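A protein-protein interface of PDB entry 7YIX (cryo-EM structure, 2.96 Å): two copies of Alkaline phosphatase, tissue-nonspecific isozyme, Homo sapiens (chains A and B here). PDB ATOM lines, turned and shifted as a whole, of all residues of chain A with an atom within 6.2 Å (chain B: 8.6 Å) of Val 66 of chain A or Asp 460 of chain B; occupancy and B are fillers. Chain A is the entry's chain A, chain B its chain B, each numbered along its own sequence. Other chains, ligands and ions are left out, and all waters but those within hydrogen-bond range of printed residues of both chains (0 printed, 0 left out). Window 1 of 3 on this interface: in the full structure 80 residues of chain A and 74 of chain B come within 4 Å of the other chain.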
ATOM      1  N   MET A  64      25.407  -8.788 -25.198  1.00  0.00           N
ATOM      2  CA  MET A  64      25.182  -9.894 -24.270  1.00  0.00           C
ATOM      3  C   MET A  64      23.961 -10.673 -24.753  1.00  0.00           C
ATOM      4  O   MET A  64      22.823 -10.361 -24.397  1.00  0.00           O
ATOM      5  CB  MET A  64      24.994  -9.377 -22.847  1.00  0.00           C
ATOM      6  CG  MET A  64      24.809 -10.465 -21.810  1.00  0.00           C
ATOM      7  SD  MET A  64      24.616  -9.804 -20.148  1.00  0.00           S
ATOM      8  CE  MET A  64      22.973  -9.102 -20.261  1.00  0.00           C
ATOM      9  N   GLY A  65      24.204 -11.699 -25.563  1.00  0.00           N
ATOM     10  CA  GLY A  65      23.143 -12.535 -26.090  1.00  0.00           C
ATOM     11  C   GLY A  65      22.666 -13.554 -25.082  1.00  0.00           C
ATOM     12  O   GLY A  65      22.501 -13.261 -23.893  1.00  0.00           O
ATOM     13  N   VAL A  66      22.422 -14.770 -25.563  1.00  0.00           N
ATOM     14  CA  VAL A  66      22.045 -15.886 -24.707  1.00  0.00           C
ATOM     15  C   VAL A  66      23.219 -16.826 -24.463  1.00  0.00           C
ATOM     16  O   VAL A  66      23.393 -17.333 -23.353  1.00  0.00           O
ATOM     17  CB  VAL A  66      20.841 -16.639 -25.313  1.00  0.00           C
ATOM     18  CG1 VAL A  66      20.432 -17.792 -24.419  1.00  0.00           C
ATOM     19  CG2 VAL A  66      19.676 -15.689 -25.522  1.00  0.00           C
ATOM     20  N   SER A  67      24.037 -17.060 -25.492  1.00  0.00           N
ATOM     21  CA  SER A  67      25.248 -17.852 -25.307  1.00  0.00           C
ATOM     22  C   SER A  67      26.201 -17.173 -24.334  1.00  0.00           C
ATOM     23  O   SER A  67      26.837 -17.839 -23.508  1.00  0.00           O
ATOM     24  CB  SER A  67      25.930 -18.089 -26.652  1.00  0.00           C
ATOM     25  OG  SER A  67      26.166 -16.865 -27.322  1.00  0.00           O
ATOM     26  N   THR A  68      26.315 -15.845 -24.419  1.00  0.00           N
ATOM     27  CA  THR A  68      27.151 -15.116 -23.472  1.00  0.00           C
ATOM     28  C   THR A  68      26.622 -15.252 -22.052  1.00  0.00           C
ATOM     29  O   THR A  68      27.400 -15.416 -21.108  1.00  0.00           O
ATOM     30  CB  THR A  68      27.243 -13.645 -23.870  1.00  0.00           C
ATOM     31  OG1 THR A  68      27.627 -13.544 -25.245  1.00  0.00           O
ATOM     32  CG2 THR A  68      28.273 -12.931 -23.013  1.00  0.00           C
ATOM     33  N   VAL A  69      25.300 -15.188 -21.878  1.00  0.00           N
ATOM     34  CA  VAL A  69      24.718 -15.338 -20.547  1.00  0.00           C
ATOM     35  C   VAL A  69      25.000 -16.730 -19.993  1.00  0.00           C
ATOM     36  O   VAL A  69      25.373 -16.884 -18.824  1.00  0.00           O
ATOM     37  CB  VAL A  69      23.210 -15.035 -20.585  1.00  0.00           C
ATOM     38  CG1 VAL A  69      22.528 -15.574 -19.342  1.00  0.00           C
ATOM     39  CG2 VAL A  69      22.977 -13.545 -20.711  1.00  0.00           C
ATOM     40  N   THR A  70      24.825 -17.765 -20.819  1.00  0.00           N
ATOM     41  CA  THR A  70      25.089 -19.126 -20.357  1.00  0.00           C
ATOM     42  C   THR A  70      26.558 -19.315 -19.990  1.00  0.00           C
ATOM     43  O   THR A  70      26.879 -19.910 -18.950  1.00  0.00           O
ATOM     44  CB  THR A  70      24.673 -20.129 -21.429  1.00  0.00           C
ATOM     45  OG1 THR A  70      23.265 -20.016 -21.668  1.00  0.00           O
ATOM     46  CG2 THR A  70      24.990 -21.543 -20.983  1.00  0.00           C
ATOM     47  N   ALA A  71      27.468 -18.815 -20.830  1.00  0.00           N
ATOM     48  CA  ALA A  71      28.890 -18.943 -20.538  1.00  0.00           C
ATOM     49  C   ALA A  71      29.265 -18.176 -19.278  1.00  0.00           C
ATOM     50  O   ALA A  71      30.091 -18.640 -18.484  1.00  0.00           O
ATOM     51  CB  ALA A  71      29.714 -18.463 -21.730  1.00  0.00           C
ATOM     52  N   ARG A  73      27.275 -17.615 -16.736  1.00  0.00           N
ATOM     53  CA  ARG A  73      26.771 -18.402 -15.615  1.00  0.00           C
ATOM     54  C   ARG A  73      27.714 -19.549 -15.278  1.00  0.00           C
ATOM     55  O   ARG A  73      28.023 -19.787 -14.103  1.00  0.00           O
ATOM     56  CB  ARG A  73      25.377 -18.937 -15.933  1.00  0.00           C
ATOM     57  CG  ARG A  73      24.740 -19.706 -14.796  1.00  0.00           C
ATOM     58  CD  ARG A  73      23.304 -20.080 -15.111  1.00  0.00           C
ATOM     59  NE  ARG A  73      23.213 -21.038 -16.206  1.00  0.00           N
ATOM     60  CZ  ARG A  73      22.543 -20.830 -17.331  1.00  0.00           C
ATOM     61  NH1 ARG A  73      21.884 -19.703 -17.544  1.00  0.00           N
ATOM     62  NH2 ARG A  73      22.529 -21.778 -18.262  1.00  0.00           N
ATOM     63  N   ASP A  92      19.111 -14.205 -13.149  1.00  0.00           N
ATOM     64  CA  ASP A  92      18.260 -15.370 -13.348  1.00  0.00           C
ATOM     65  C   ASP A  92      17.140 -15.451 -12.322  1.00  0.00           C
ATOM     66  O   ASP A  92      16.173 -16.189 -12.537  1.00  0.00           O
ATOM     67  CB  ASP A  92      19.091 -16.652 -13.296  1.00  0.00           C
ATOM     68  CG  ASP A  92      19.762 -16.964 -14.615  1.00  0.00           C
ATOM     69  OD1 ASP A  92      19.742 -16.095 -15.512  1.00  0.00           O
ATOM     70  OD2 ASP A  92      20.310 -18.076 -14.754  1.00  0.00           O
ATOM     71  N   LEU A  99      11.558 -11.554 -25.089  1.00  0.00           N
ATOM     72  CA  LEU A  99      12.495 -11.525 -26.203  1.00  0.00           C
ATOM     73  C   LEU A  99      12.255 -10.288 -27.058  1.00  0.00           C
ATOM     74  O   LEU A  99      11.113  -9.863 -27.261  1.00  0.00           O
ATOM     75  CB  LEU A  99      12.377 -12.781 -27.071  1.00  0.00           C
ATOM     76  CG  LEU A  99      13.127 -14.030 -26.605  1.00  0.00           C
ATOM     77  CD1 LEU A  99      12.443 -15.277 -27.123  1.00  0.00           C
ATOM     78  CD2 LEU A  99      14.571 -13.992 -27.064  1.00  0.00           C
ATOM     79  N   SER A 382      23.563  -9.083 -30.055  1.00  0.00           N
ATOM     80  CA  SER A 382      24.340 -10.266 -29.720  1.00  0.00           C
ATOM     81  C   SER A 382      25.436 -10.452 -30.761  1.00  0.00           C
ATOM     82  O   SER A 382      25.409  -9.850 -31.837  1.00  0.00           O
ATOM     83  CB  SER A 382      23.454 -11.513 -29.637  1.00  0.00           C
ATOM     84  OG  SER A 382      22.878 -11.812 -30.894  1.00  0.00           O
ATOM     85  N   ASP A 460      17.784 -12.633 -31.709  1.00  0.00           N
ATOM     86  CA  ASP A 460      16.962 -11.902 -30.758  1.00  0.00           C
ATOM     87  C   ASP A 460      17.642 -11.866 -29.395  1.00  0.00           C
ATOM     88  O   ASP A 460      18.444 -12.736 -29.048  1.00  0.00           O
ATOM     89  CB  ASP A 460      15.583 -12.545 -30.637  1.00  0.00           C
ATOM     90  CG  ASP A 460      14.716 -12.288 -31.847  1.00  0.00           C
ATOM     91  OD1 ASP A 460      15.073 -11.401 -32.650  1.00  0.00           O
ATOM     92  OD2 ASP A 460      13.683 -12.974 -31.999  1.00  0.00           O
ATOM     93  N   VAL A 461      17.316 -10.842 -28.611  1.00  0.00           N
ATOM     94  CA  VAL A 461      17.959 -10.666 -27.315  1.00  0.00           C
ATOM     95  C   VAL A 461      16.938 -10.902 -26.213  1.00  0.00           C
ATOM     96  O   VAL A 461      15.727 -10.858 -26.443  1.00  0.00           O
ATOM     97  CB  VAL A 461      18.608  -9.273 -27.176  1.00  0.00           C
ATOM     98  CG1 VAL A 461      19.716  -9.111 -28.192  1.00  0.00           C
ATOM     99  CG2 VAL A 461      17.568  -8.185 -27.340  1.00  0.00           C
ATOM    100  N   ALA A 462      17.435 -11.166 -25.010  1.00  0.00           N
ATOM    101  CA  ALA A 462      16.586 -11.466 -23.866  1.00  0.00           C
ATOM    102  C   ALA A 462      16.510 -10.265 -22.936  1.00  0.00           C
ATOM    103  O   ALA A 462      17.509  -9.576 -22.710  1.00  0.00           O
ATOM    104  CB  ALA A 462      17.107 -12.685 -23.105  1.00  0.00           C
ATOM    105  N   MET B  64      16.360 -26.476 -32.391  1.00  0.00           N
ATOM    106  CA  MET B  64      15.862 -25.169 -32.811  1.00  0.00           C
ATOM    107  C   MET B  64      16.156 -24.170 -31.696  1.00  0.00           C
ATOM    108  O   MET B  64      15.361 -24.010 -30.766  1.00  0.00           O
ATOM    109  CB  MET B  64      14.371 -25.236 -33.126  1.00  0.00           C
ATOM    110  CG  MET B  64      13.776 -23.937 -33.622  1.00  0.00           C
ATOM    111  SD  MET B  64      12.024 -24.095 -33.996  1.00  0.00           S
ATOM    112  CE  MET B  64      11.343 -24.223 -32.345  1.00  0.00           C
ATOM    113  N   GLY B  65      17.296 -23.495 -31.794  1.00  0.00           N
ATOM    114  CA  GLY B  65      17.705 -22.559 -30.767  1.00  0.00           C
ATOM    115  C   GLY B  65      17.044 -21.203 -30.893  1.00  0.00           C
ATOM    116  O   GLY B  65      15.834 -21.115 -31.116  1.00  0.00           O
ATOM    117  N   VAL B  66      17.829 -20.139 -30.740  1.00  0.00           N
ATOM    118  CA  VAL B  66      17.324 -18.785 -30.881  1.00  0.00           C
ATOM    119  C   VAL B  66      17.779 -18.128 -32.181  1.00  0.00           C
ATOM    120  O   VAL B  66      17.080 -17.245 -32.693  1.00  0.00           O
ATOM    121  CB  VAL B  66      17.727 -17.927 -29.662  1.00  0.00           C
ATOM    122  CG1 VAL B  66      17.048 -16.571 -29.702  1.00  0.00           C
ATOM    123  CG2 VAL B  66      17.385 -18.653 -28.373  1.00  0.00           C
ATOM    124  N   SER B  67      18.923 -18.532 -32.736  1.00  0.00           N
ATOM    125  CA  SER B  67      19.313 -18.042 -34.054  1.00  0.00           C
ATOM    126  C   SER B  67      18.500 -18.716 -35.151  1.00  0.00           C
ATOM    127  O   SER B  67      18.169 -18.091 -36.167  1.00  0.00           O
ATOM    128  CB  SER B  67      20.805 -18.269 -34.277  1.00  0.00           C
ATOM    129  OG  SER B  67      21.271 -17.506 -35.374  1.00  0.00           O
ATOM    130  N   ALA B  98       9.436 -18.349 -22.098  1.00  0.00           N
ATOM    131  CA  ALA B  98      10.351 -18.633 -21.004  1.00  0.00           C
ATOM    132  C   ALA B  98      11.649 -19.202 -21.561  1.00  0.00           C
ATOM    133  O   ALA B  98      11.760 -19.501 -22.750  1.00  0.00           O
ATOM    134  CB  ALA B  98       9.732 -19.606 -19.992  1.00  0.00           C
ATOM    135  N   LEU B  99      12.636 -19.359 -20.682  1.00  0.00           N
ATOM    136  CA  LEU B  99      13.939 -19.894 -21.049  1.00  0.00           C
ATOM    137  C   LEU B  99      14.218 -21.161 -20.256  1.00  0.00           C
ATOM    138  O   LEU B  99      13.898 -21.245 -19.066  1.00  0.00           O
ATOM    139  CB  LEU B  99      15.051 -18.871 -20.803  1.00  0.00           C
ATOM    140  CG  LEU B  99      15.274 -17.799 -21.870  1.00  0.00           C
ATOM    141  CD1 LEU B  99      16.257 -16.761 -21.371  1.00  0.00           C
ATOM    142  CD2 LEU B  99      15.769 -18.415 -23.161  1.00  0.00           C
ATOM    143  N   SER B 100      14.820 -22.144 -20.920  1.00  0.00           N
ATOM    144  CA  SER B 100      15.088 -23.449 -20.336  1.00  0.00           C
ATOM    145  C   SER B 100      16.578 -23.746 -20.405  1.00  0.00           C
ATOM    146  O   SER B 100      17.208 -23.549 -21.452  1.00  0.00           O
ATOM    147  CB  SER B 100      14.299 -24.546 -21.054  1.00  0.00           C
ATOM    148  OG  SER B 100      12.934 -24.517 -20.680  1.00  0.00           O
ATOM    149  N   LYS B 101      17.127 -24.216 -19.286  1.00  0.00           N
ATOM    150  CA  LYS B 101      18.511 -24.668 -19.213  1.00  0.00           C
ATOM    151  C   LYS B 101      18.576 -26.141 -19.591  1.00  0.00           C
ATOM    152  O   LYS B 101      17.813 -26.957 -19.065  1.00  0.00           O
ATOM    153  CB  LYS B 101      19.082 -24.454 -17.813  1.00  0.00           C
ATOM    154  CG  LYS B 101      18.586 -23.197 -17.128  1.00  0.00           C
ATOM    155  CD  LYS B 101      19.579 -22.701 -16.094  1.00  0.00           C
ATOM    156  CE  LYS B 101      19.440 -23.461 -14.790  1.00  0.00           C
ATOM    157  NZ  LYS B 101      19.793 -22.613 -13.622  1.00  0.00           N
ATOM    158  N   THR B 102      19.498 -26.481 -20.489  1.00  0.00           N
ATOM    159  CA  THR B 102      19.484 -27.792 -21.124  1.00  0.00           C
ATOM    160  C   THR B 102      20.748 -28.598 -20.856  1.00  0.00           C
ATOM    161  O   THR B 102      21.330 -29.155 -21.788  1.00  0.00           O
ATOM    162  CB  THR B 102      19.298 -27.647 -22.636  1.00  0.00           C
ATOM    163  OG1 THR B 102      20.531 -27.222 -23.230  1.00  0.00           O
ATOM    164  CG2 THR B 102      18.223 -26.625 -22.947  1.00  0.00           C
ATOM    165  N   TYR B 103      21.193 -28.666 -19.608  1.00  0.00           N
ATOM    166  CA  TYR B 103      22.350 -29.480 -19.264  1.00  0.00           C
ATOM    167  C   TYR B 103      21.901 -30.847 -18.764  1.00  0.00           C
ATOM    168  O   TYR B 103      20.829 -30.990 -18.172  1.00  0.00           O
ATOM    169  CB  TYR B 103      23.216 -28.793 -18.205  1.00  0.00           C
ATOM    170  CG  TYR B 103      22.607 -28.769 -16.821  1.00  0.00           C
ATOM    171  CD1 TYR B 103      21.646 -27.830 -16.481  1.00  0.00           C
ATOM    172  CD2 TYR B 103      23.001 -29.680 -15.852  1.00  0.00           C
ATOM    173  CE1 TYR B 103      21.089 -27.804 -15.223  1.00  0.00           C
ATOM    174  CE2 TYR B 103      22.448 -29.662 -14.590  1.00  0.00           C
ATOM    175  CZ  TYR B 103      21.494 -28.722 -14.281  1.00  0.00           C
ATOM    176  OH  TYR B 103      20.942 -28.698 -13.023  1.00  0.00           O
ATOM    177  N   PRO B 110      24.257 -30.785 -24.113  1.00  0.00           N
ATOM    178  CA  PRO B 110      23.201 -31.804 -24.039  1.00  0.00           C
ATOM    179  C   PRO B 110      23.227 -32.843 -25.148  1.00  0.00           C
ATOM    180  O   PRO B 110      24.085 -32.825 -26.034  1.00  0.00           O
ATOM    181  CB  PRO B 110      21.916 -30.974 -24.118  1.00  0.00           C
ATOM    182  CG  PRO B 110      22.321 -29.715 -24.795  1.00  0.00           C
ATOM    183  CD  PRO B 110      23.708 -29.437 -24.326  1.00  0.00           C
ATOM    184  N   ALA B 379      11.999 -26.710 -27.623  1.00  0.00           N
ATOM    185  CA  ALA B 379      13.135 -27.359 -28.256  1.00  0.00           C
ATOM    186  C   ALA B 379      13.957 -28.044 -27.176  1.00  0.00           C
ATOM    187  O   ALA B 379      13.808 -27.761 -25.985  1.00  0.00           O
ATOM    188  CB  ALA B 379      13.998 -26.363 -29.034  1.00  0.00           C
ATOM    189  N   ASP B 380      14.829 -28.956 -27.599  1.00  0.00           N
ATOM    190  CA  ASP B 380      15.632 -29.719 -26.653  1.00  0.00           C
ATOM    191  C   ASP B 380      17.072 -29.238 -26.539  1.00  0.00           C
ATOM    192  O   ASP B 380      17.672 -29.379 -25.469  1.00  0.00           O
ATOM    193  CB  ASP B 380      15.614 -31.205 -27.024  1.00  0.00           C
ATOM    194  CG  ASP B 380      16.126 -31.466 -28.416  1.00  0.00           C
ATOM    195  OD1 ASP B 380      16.137 -30.523 -29.230  1.00  0.00           O
ATOM    196  OD2 ASP B 380      16.513 -32.617 -28.699  1.00  0.00           O
ATOM    197  N   HIS B 381      17.641 -28.672 -27.598  1.00  0.00           N
ATOM    198  CA  HIS B 381      18.998 -28.138 -27.550  1.00  0.00           C
ATOM    199  C   HIS B 381      19.148 -27.110 -28.666  1.00  0.00           C
ATOM    200  O   HIS B 381      18.163 -26.673 -29.268  1.00  0.00           O
ATOM    201  CB  HIS B 381      20.037 -29.259 -27.660  1.00  0.00           C
ATOM    202  CG  HIS B 381      19.855 -30.135 -28.858  1.00  0.00           C
ATOM    203  ND1 HIS B 381      19.138 -31.310 -28.817  1.00  0.00           N
ATOM    204  CD2 HIS B 381      20.286 -30.000 -30.133  1.00  0.00           C
ATOM    205  CE1 HIS B 381      19.140 -31.866 -30.015  1.00  0.00           C
ATOM    206  NE2 HIS B 381      19.829 -31.091 -30.832  1.00  0.00           N
ATOM    207  N   SER B 382      20.390 -26.715 -28.935  1.00  0.00           N
ATOM    208  CA  SER B 382      20.686 -25.759 -29.991  1.00  0.00           C
ATOM    209  C   SER B 382      22.042 -26.094 -30.589  1.00  0.00           C
ATOM    210  O   SER B 382      22.838 -26.830 -30.000  1.00  0.00           O
ATOM    211  CB  SER B 382      20.666 -24.320 -29.472  1.00  0.00           C
ATOM    212  OG  SER B 382      21.698 -24.106 -28.529  1.00  0.00           O
ATOM    213  N   HIS B 383      22.297 -25.550 -31.772  1.00  0.00           N
ATOM    214  CA  HIS B 383      23.513 -25.813 -32.524  1.00  0.00           C
ATOM    215  C   HIS B 383      24.422 -24.586 -32.490  1.00  0.00           C
ATOM    216  O   HIS B 383      24.150 -23.599 -31.802  1.00  0.00           O
ATOM    217  CB  HIS B 383      23.171 -26.210 -33.960  1.00  0.00           C
ATOM    218  CG  HIS B 383      22.624 -27.596 -34.087  1.00  0.00           C
ATOM    219  ND1 HIS B 383      23.403 -28.674 -34.446  1.00  0.00           N
ATOM    220  CD2 HIS B 383      21.374 -28.080 -33.904  1.00  0.00           C
ATOM    221  CE1 HIS B 383      22.656 -29.763 -34.479  1.00  0.00           C
ATOM    222  NE2 HIS B 383      21.421 -29.429 -34.153  1.00  0.00           N
ATOM    223  N   GLY B 457      25.108 -27.367 -29.080  1.00  0.00           N
ATOM    224  CA  GLY B 457      25.488 -26.158 -28.381  1.00  0.00           C
ATOM    225  C   GLY B 457      24.855 -26.117 -27.005  1.00  0.00           C
ATOM    226  O   GLY B 457      23.806 -26.718 -26.757  1.00  0.00           O
ATOM    227  N   GLY B 458      25.513 -25.392 -26.108  1.00  0.00           N
ATOM    228  CA  GLY B 458      25.106 -25.307 -24.722  1.00  0.00           C
ATOM    229  C   GLY B 458      24.166 -24.174 -24.373  1.00  0.00           C
ATOM    230  O   GLY B 458      23.904 -23.957 -23.184  1.00  0.00           O
ATOM    231  N   GLU B 459      23.646 -23.448 -25.358  1.00  0.00           N
ATOM    232  CA  GLU B 459      22.800 -22.298 -25.079  1.00  0.00           C
ATOM    233  C   GLU B 459      21.463 -22.727 -24.484  1.00  0.00           C
ATOM    234  O   GLU B 459      20.996 -23.850 -24.690  1.00  0.00           O
ATOM    235  CB  GLU B 459      22.553 -21.494 -26.354  1.00  0.00           C
ATOM    236  CG  GLU B 459      23.795 -20.860 -26.947  1.00  0.00           C
ATOM    237  CD  GLU B 459      24.530 -21.781 -27.900  1.00  0.00           C
ATOM    238  OE1 GLU B 459      24.033 -22.897 -28.149  1.00  0.00           O
ATOM    239  OE2 GLU B 459      25.604 -21.389 -28.403  1.00  0.00           O
ATOM    240  N   ASP B 460      20.849 -21.816 -23.733  1.00  0.00           N
ATOM    241  CA  ASP B 460      19.492 -22.030 -23.258  1.00  0.00           C
ATOM    242  C   ASP B 460      18.509 -21.934 -24.420  1.00  0.00           C
ATOM    243  O   ASP B 460      18.766 -21.276 -25.431  1.00  0.00           O
ATOM    244  CB  ASP B 460      19.129 -21.009 -22.183  1.00  0.00           C
ATOM    245  CG  ASP B 460      20.102 -21.014 -21.027  1.00  0.00           C
ATOM    246  OD1 ASP B 460      20.925 -21.949 -20.950  1.00  0.00           O
ATOM    247  OD2 ASP B 460      20.044 -20.085 -20.192  1.00  0.00           O
ATOM    248  N   VAL B 461      17.367 -22.597 -24.268  1.00  0.00           N
ATOM    249  CA  VAL B 461      16.387 -22.651 -25.345  1.00  0.00           C
ATOM    250  C   VAL B 461      15.145 -21.879 -24.929  1.00  0.00           C
ATOM    251  O   VAL B 461      14.916 -21.622 -23.744  1.00  0.00           O
ATOM    252  CB  VAL B 461      16.028 -24.102 -25.726  1.00  0.00           C
ATOM    253  CG1 VAL B 461      17.244 -24.810 -26.285  1.00  0.00           C
ATOM    254  CG2 VAL B 461      15.478 -24.845 -24.527  1.00  0.00           C
ATOM    255  N   ALA B 462      14.345 -21.494 -25.918  1.00  0.00           N
ATOM    256  CA  ALA B 462      13.137 -20.721 -25.671  1.00  0.00           C
ATOM    257  C   ALA B 462      11.914 -21.625 -25.705  1.00  0.00           C
ATOM    258  O   ALA B 462      11.836 -22.557 -26.509  1.00  0.00           O
ATOM    259  CB  ALA B 462      12.992 -19.602 -26.702  1.00  0.00           C
ATOM    260  N   VAL B 463      10.957 -21.343 -24.825  1.00  0.00           N
ATOM    261  CA  VAL B 463       9.730 -22.120 -24.705  1.00  0.00           C
ATOM    262  C   VAL B 463       8.554 -21.166 -24.857  1.00  0.00           C
ATOM    263  O   VAL B 463       8.389 -20.249 -24.044  1.00  0.00           O
ATOM    264  CB  VAL B 463       9.652 -22.862 -23.361  1.00  0.00           C
ATOM    265  CG1 VAL B 463       8.250 -23.388 -23.118  1.00  0.00           C
ATOM    266  CG2 VAL B 463      10.665 -23.990 -23.319  1.00  0.00           C
ATOM    267  N   GLY B 475       9.945 -17.582 -16.136  1.00  0.00           N
ATOM    268  CA  GLY B 475      11.320 -17.139 -16.010  1.00  0.00           C
ATOM    269  C   GLY B 475      12.338 -18.031 -16.689  1.00  0.00           C
ATOM    270  O   GLY B 475      12.037 -18.666 -17.702  1.00  0.00           O
ATOM    271  N   VAL B 476      13.549 -18.073 -16.145  1.00  0.00           N
ATOM    272  CA  VAL B 476      14.603 -18.967 -16.611  1.00  0.00           C
ATOM    273  C   VAL B 476      14.629 -20.156 -15.662  1.00  0.00           C
ATOM    274  O   VAL B 476      14.948 -20.005 -14.478  1.00  0.00           O
ATOM    275  CB  VAL B 476      15.965 -18.265 -16.657  1.00  0.00           C
ATOM    276  CG1 VAL B 476      17.066 -19.269 -16.954  1.00  0.00           C
ATOM    277  CG2 VAL B 476      15.956 -17.155 -17.687  1.00  0.00           C
ATOM    278  N   HIS B 477      14.303 -21.342 -16.171  1.00  0.00           N
ATOM    279  CA  HIS B 477      14.121 -22.505 -15.315  1.00  0.00           C
ATOM    280  C   HIS B 477      14.779 -23.721 -15.951  1.00  0.00           C
ATOM    281  O   HIS B 477      15.345 -23.651 -17.045  1.00  0.00           O
ATOM    282  CB  HIS B 477      12.634 -22.761 -15.048  1.00  0.00           C
ATOM    283  CG  HIS B 477      11.789 -22.751 -16.283  1.00  0.00           C
ATOM    284  ND1 HIS B 477      11.973 -23.643 -17.318  1.00  0.00           N
ATOM    285  CD2 HIS B 477      10.749 -21.965 -16.646  1.00  0.00           C
ATOM    286  CE1 HIS B 477      11.087 -23.402 -18.267  1.00  0.00           C
ATOM    287  NE2 HIS B 477      10.333 -22.389 -17.884  1.00  0.00           N
ATOM    288  N   GLN B 479      14.787 -27.715 -17.475  1.00  0.00           N
ATOM    289  CA  GLN B 479      13.980 -28.355 -18.508  1.00  0.00           C
ATOM    290  C   GLN B 479      12.905 -29.247 -17.901  1.00  0.00           C
ATOM    291  O   GLN B 479      11.756 -29.244 -18.362  1.00  0.00           O
ATOM    292  CB  GLN B 479      14.878 -29.155 -19.447  1.00  0.00           C
ATOM    293  CG  GLN B 479      14.421 -29.145 -20.890  1.00  0.00           C
ATOM    294  CD  GLN B 479      15.532 -29.503 -21.848  1.00  0.00           C
ATOM    295  OE1 GLN B 479      16.322 -30.408 -21.588  1.00  0.00           O
ATOM    296  NE2 GLN B 479      15.600 -28.794 -22.967  1.00  0.00           N
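Val 66 of chain A touches Asp 460 of chain B. Ser 67 of chain A touches Glu 459 of chain B (CB to CG, 3.5 Å). Thr 70 of chain A touches Gly 458 of chain B (CG2 to O, 3.4 Å). Arg 73 of chain A touches Lys 101 of chain B.
The backbone carbonyl oxygen (O) of Val 66 of chain A sits at hydrogen-bond distance from the side-chain hydroxyl (OG1) of Thr 70 of chain A (3.2 Å). The guanidinium group (NH1) of Arg 73 of chain A is in salt-bridge range of the side-chain carboxylate (OD2) of Asp 92 of chain A, 3.6 Å away. N of Lys 101 of chain B sits at hydrogen-bond distance from O of His 477 of chain B (2.9 Å). The side-chain hydroxyl (OG) of Ser 382 of chain B sits at hydrogen-bond distance from the side-chain carboxylate (OE1) of Glu 459 of chain B, 2.7 Å away.
The side-chain hydroxyl of Thr 70 of chain A lies within hydrogen-bond range of the side-chain carboxylate of Asp 460 of chain B (3.1 Å). The guanidinium group of Arg 73 of chain A lies within salt-bridge range of the side-chain carboxylate of Asp 460 of chain B (3.1 Å).
Of the 15 printed residues of chain A, 4 touch a printed residue of chain B. Hydrophobic or aromatic side chains of chain A within 4 Å of the printed part of chain B: Val 66. Printed residues of chain B that touch a printed residue of chain A: Lys 101, Gly 458, Glu 459 and Asp 460. Among the printed residues, 6 pairs touch across the chains.
No residue of chain B comes within 4 Å of Gly 65 of chain A. Of the printed residues of chain B, Val 66 of chain A touches Asp 460. Ala 462 of chain A touches none of the printed residues of chain B. Of the printed residues of chain A, Lys 101 of chain B touches Arg 73 (3.7 Å). Printed residues of chain A within 4 Å of Gly 458 of chain B: Thr 70 (3.4 Å). Of the printed residues of chain A, Glu 459 of chain B touches Ser 67. Of the printed residues of chain A, Asp 460 of chain B touches Val 66 (3.99 Å), Thr 70 (3.1 Å) and Arg 73 (3.1 Å).
Val 66 of chain A touches Asp 460 of chain B, but with the chains exchanged Asp 460 of chain A does not touch Val 66 of chain B (4.1 Å).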
